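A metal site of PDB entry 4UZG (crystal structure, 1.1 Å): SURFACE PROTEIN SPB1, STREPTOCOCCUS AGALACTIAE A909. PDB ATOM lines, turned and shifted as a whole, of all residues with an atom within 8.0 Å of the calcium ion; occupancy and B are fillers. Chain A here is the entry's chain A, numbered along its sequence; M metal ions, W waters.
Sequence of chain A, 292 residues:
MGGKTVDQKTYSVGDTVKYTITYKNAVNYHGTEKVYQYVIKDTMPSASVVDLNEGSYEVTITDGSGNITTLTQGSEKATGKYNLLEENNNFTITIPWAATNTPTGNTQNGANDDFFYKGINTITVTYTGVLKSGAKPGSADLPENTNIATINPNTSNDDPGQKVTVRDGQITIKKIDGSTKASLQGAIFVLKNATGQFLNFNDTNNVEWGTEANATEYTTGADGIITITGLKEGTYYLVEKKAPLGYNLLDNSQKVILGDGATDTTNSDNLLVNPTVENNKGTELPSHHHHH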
ATOM      1  N   SER A  12      26.775 -27.897   6.134  1.00  0.00           N
ATOM      2  CA  SER A  12      25.678 -26.940   6.150  1.00  0.00           C
ATOM      3  C   SER A  12      25.703 -26.162   7.452  1.00  0.00           C
ATOM      4  O   SER A  12      26.103 -26.669   8.502  1.00  0.00           O
ATOM      5  CB  SER A  12      24.310 -27.625   6.032  1.00  0.00           C
ATOM      6  OG  SER A  12      24.107 -28.124   4.723  1.00  0.00           O
ATOM      7  N   VAL A  13      25.251 -24.901   7.384  1.00  0.00           N
ATOM      8  CA  VAL A  13      25.046 -24.102   8.568  1.00  0.00           C
ATOM      9  C   VAL A  13      24.202 -24.877   9.578  1.00  0.00           C
ATOM     10  O   VAL A  13      23.195 -25.501   9.215  1.00  0.00           O
ATOM     11  CB  VAL A  13      24.445 -22.744   8.170  1.00  0.00           C
ATOM     12  CG1 VAL A  13      23.889 -22.001   9.378  1.00  0.00           C
ATOM     13  CG2 VAL A  13      25.496 -21.898   7.456  1.00  0.00           C
ATOM     14  N   GLY A  14      24.649 -24.876  10.824  1.00  0.00           N
ATOM     15  CA  GLY A  14      24.046 -25.643  11.900  1.00  0.00           C
ATOM     16  C   GLY A  14      24.689 -26.995  12.188  1.00  0.00           C
ATOM     17  O   GLY A  14      24.411 -27.590  13.233  1.00  0.00           O
ATOM     18  N   ASP A  15      25.522 -27.461  11.277  1.00  0.00           N
ATOM     19  CA  ASP A  15      26.168 -28.758  11.456  1.00  0.00           C
ATOM     20  C   ASP A  15      27.224 -28.701  12.574  1.00  0.00           C
ATOM     21  O   ASP A  15      27.842 -27.668  12.850  1.00  0.00           O
ATOM     22  CB  ASP A  15      26.900 -29.222  10.188  1.00  0.00           C
ATOM     23  CG  ASP A  15      25.993 -29.727   9.080  1.00  0.00           C
ATOM     24  OD1 ASP A  15      24.762 -29.805   9.243  1.00  0.00           O
ATOM     25  OD2 ASP A  15      26.583 -30.056   8.025  1.00  0.00           O
ATOM     26  N   THR A  16      27.421 -29.848  13.188  1.00  0.00           N
ATOM     27  CA  THR A  16      28.538 -30.073  14.099  1.00  0.00           C
ATOM     28  C   THR A  16      29.797 -30.333  13.285  1.00  0.00           C
ATOM     29  O   THR A  16      29.831 -31.234  12.432  1.00  0.00           O
ATOM     30  CB  THR A  16      28.251 -31.266  15.006  1.00  0.00           C
ATOM     31  OG1 THR A  16      27.071 -30.977  15.753  1.00  0.00           O
ATOM     32  CG2 THR A  16      29.412 -31.521  15.964  1.00  0.00           C
ATOM     33  N   VAL A 130      29.929 -25.636  16.176  1.00  0.00           N
ATOM     34  CA  VAL A 130      28.728 -25.592  15.344  1.00  0.00           C
ATOM     35  C   VAL A 130      28.850 -24.457  14.340  1.00  0.00           C
ATOM     36  O   VAL A 130      29.121 -23.310  14.709  1.00  0.00           O
ATOM     37  CB  VAL A 130      27.453 -25.442  16.205  1.00  0.00           C
ATOM     38  CG1 VAL A 130      26.217 -25.298  15.331  1.00  0.00           C
ATOM     39  CG2 VAL A 130      27.301 -26.622  17.170  1.00  0.00           C
ATOM     40  N   ASN A 200      14.224 -26.293   5.485  1.00  0.00           N
ATOM     41  CA  ASN A 200      13.705 -25.288   6.394  1.00  0.00           C
ATOM     42  C   ASN A 200      14.925 -24.543   6.932  1.00  0.00           C
ATOM     43  O   ASN A 200      15.768 -25.133   7.622  1.00  0.00           O
ATOM     44  CB  ASN A 200      12.906 -25.895   7.538  1.00  0.00           C
ATOM     45  CG  ASN A 200      12.452 -24.809   8.522  1.00  0.00           C
ATOM     46  OD1 ASN A 200      13.222 -24.004   9.010  1.00  0.00           O
ATOM     47  ND2 ASN A 200      11.158 -24.727   8.734  1.00  0.00           N
ATOM     48  N   ASN A 205      20.651 -19.795  11.769  1.00  0.00           N
ATOM     49  CA  ASN A 205      21.857 -20.523  12.168  1.00  0.00           C
ATOM     50  C   ASN A 205      21.737 -22.039  12.037  1.00  0.00           C
ATOM     51  O   ASN A 205      22.640 -22.740  12.504  1.00  0.00           O
ATOM     52  CB  ASN A 205      22.262 -20.143  13.582  1.00  0.00           C
ATOM     53  CG  ASN A 205      22.697 -18.715  13.679  1.00  0.00           C
ATOM     54  OD1 ASN A 205      23.649 -18.300  13.002  1.00  0.00           O
ATOM     55  ND2 ASN A 205      21.979 -17.928  14.496  1.00  0.00           N
ATOM     56  N   ASN A 206      20.688 -22.563  11.398  1.00  0.00           N
ATOM     57  CA  ASN A 206      20.548 -23.997  11.335  1.00  0.00           C
ATOM     58  C   ASN A 206      19.705 -24.469  10.170  1.00  0.00           C
ATOM     59  O   ASN A 206      18.468 -24.425  10.215  1.00  0.00           O
ATOM     60  CB  ASN A 206      19.974 -24.543  12.647  1.00  0.00           C
ATOM     61  CG  ASN A 206      19.922 -26.049  12.642  1.00  0.00           C
ATOM     62  OD1 ASN A 206      20.702 -26.716  11.955  1.00  0.00           O
ATOM     63  ND2 ASN A 206      19.043 -26.595  13.440  1.00  0.00           N
ATOM     64  N   VAL A 207      20.352 -24.963   9.107  1.00  0.00           N
ATOM     65  CA  VAL A 207      19.682 -25.687   8.041  1.00  0.00           C
ATOM     66  C   VAL A 207      19.018 -26.925   8.602  1.00  0.00           C
ATOM     67  O   VAL A 207      19.668 -27.691   9.322  1.00  0.00           O
ATOM     68  CB  VAL A 207      20.744 -26.109   6.985  1.00  0.00           C
ATOM     69  CG1 VAL A 207      20.251 -27.216   6.049  1.00  0.00           C
ATOM     70  CG2 VAL A 207      21.251 -24.908   6.196  1.00  0.00           C
ATOM     71  N   GLU A 208      17.749 -27.152   8.245  1.00  0.00           N
ATOM     72  CA  GLU A 208      17.048 -28.361   8.623  1.00  0.00           C
ATOM     73  C   GLU A 208      16.358 -28.932   7.396  1.00  0.00           C
ATOM     74  O   GLU A 208      16.016 -28.209   6.445  1.00  0.00           O
ATOM     75  CB  GLU A 208      16.023 -28.069   9.713  1.00  0.00           C
ATOM     76  CG  GLU A 208      16.667 -27.878  11.104  1.00  0.00           C
ATOM     77  CD  GLU A 208      17.244 -29.191  11.654  1.00  0.00           C
ATOM     78  OE1 GLU A 208      16.484 -30.200  11.776  1.00  0.00           O
ATOM     79  OE2 GLU A 208      18.453 -29.297  11.851  1.00  0.00           O
ATOM     80  N   TRP A 209      16.148 -30.242   7.422  1.00  0.00           N
ATOM     81  CA  TRP A 209      15.557 -30.992   6.323  1.00  0.00           C
ATOM     82  C   TRP A 209      14.334 -31.725   6.847  1.00  0.00           C
ATOM     83  O   TRP A 209      14.423 -32.428   7.846  1.00  0.00           O
ATOM     84  CB  TRP A 209      16.571 -31.965   5.733  1.00  0.00           C
ATOM     85  CG  TRP A 209      17.758 -31.285   5.155  1.00  0.00           C
ATOM     86  CD1 TRP A 209      19.001 -31.198   5.717  1.00  0.00           C
ATOM     87  CD2 TRP A 209      17.802 -30.531   3.942  1.00  0.00           C
ATOM     88  NE1 TRP A 209      19.815 -30.436   4.933  1.00  0.00           N
ATOM     89  CE2 TRP A 209      19.114 -30.021   3.826  1.00  0.00           C
ATOM     90  CE3 TRP A 209      16.876 -30.265   2.923  1.00  0.00           C
ATOM     91  CZ2 TRP A 209      19.511 -29.245   2.746  1.00  0.00           C
ATOM     92  CZ3 TRP A 209      17.264 -29.511   1.867  1.00  0.00           C
ATOM     93  CH2 TRP A 209      18.571 -28.998   1.773  1.00  0.00           C
HETATM   94 CA    CA M   1      20.697 -28.926  11.017  1.00  0.00          CA
HETATM   95  O   HOH W   1      20.074 -30.798   9.706  1.00  0.00           O
HETATM   96  O   HOH W   2      22.509 -30.657  11.353  1.00  0.00           O
HETATM   97  O   HOH W   3      20.982 -29.327  13.374  1.00  0.00           O
HETATM   98  O   HOH W   4      22.636 -28.160   9.920  1.00  0.00           O
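Water W4 lies within hydrogen-bond range of OD1 of Asp 15 and O of Val 13.
Of the 12 residues printed, 3 come within 4 Å of the calcium ion.
Along chain A the residues within 4 Å of the calcium ion span positions 206 to 208.
The calcium ion is bound by the backbone carbonyl oxygen (O) of Val 207 (2.3 Å), water W4 (2.4 Å), water W1 (2.4 Å), the side-chain amide oxygen (OD1) of Asn 206 (2.4 Å), water W3 (2.4 Å), the side-chain carboxylate (OE2) of Glu 208 (2.4 Å) and water W2 (2.5 Å).
The backbone NH (N) of Val 207 lies within hydrogen-bond range of the backbone carbonyl oxygen (O) of Val 13 (2.9 Å).
O of Glu 208 sits at hydrogen-bond distance from N of Asn 200, 2.8 Å away.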
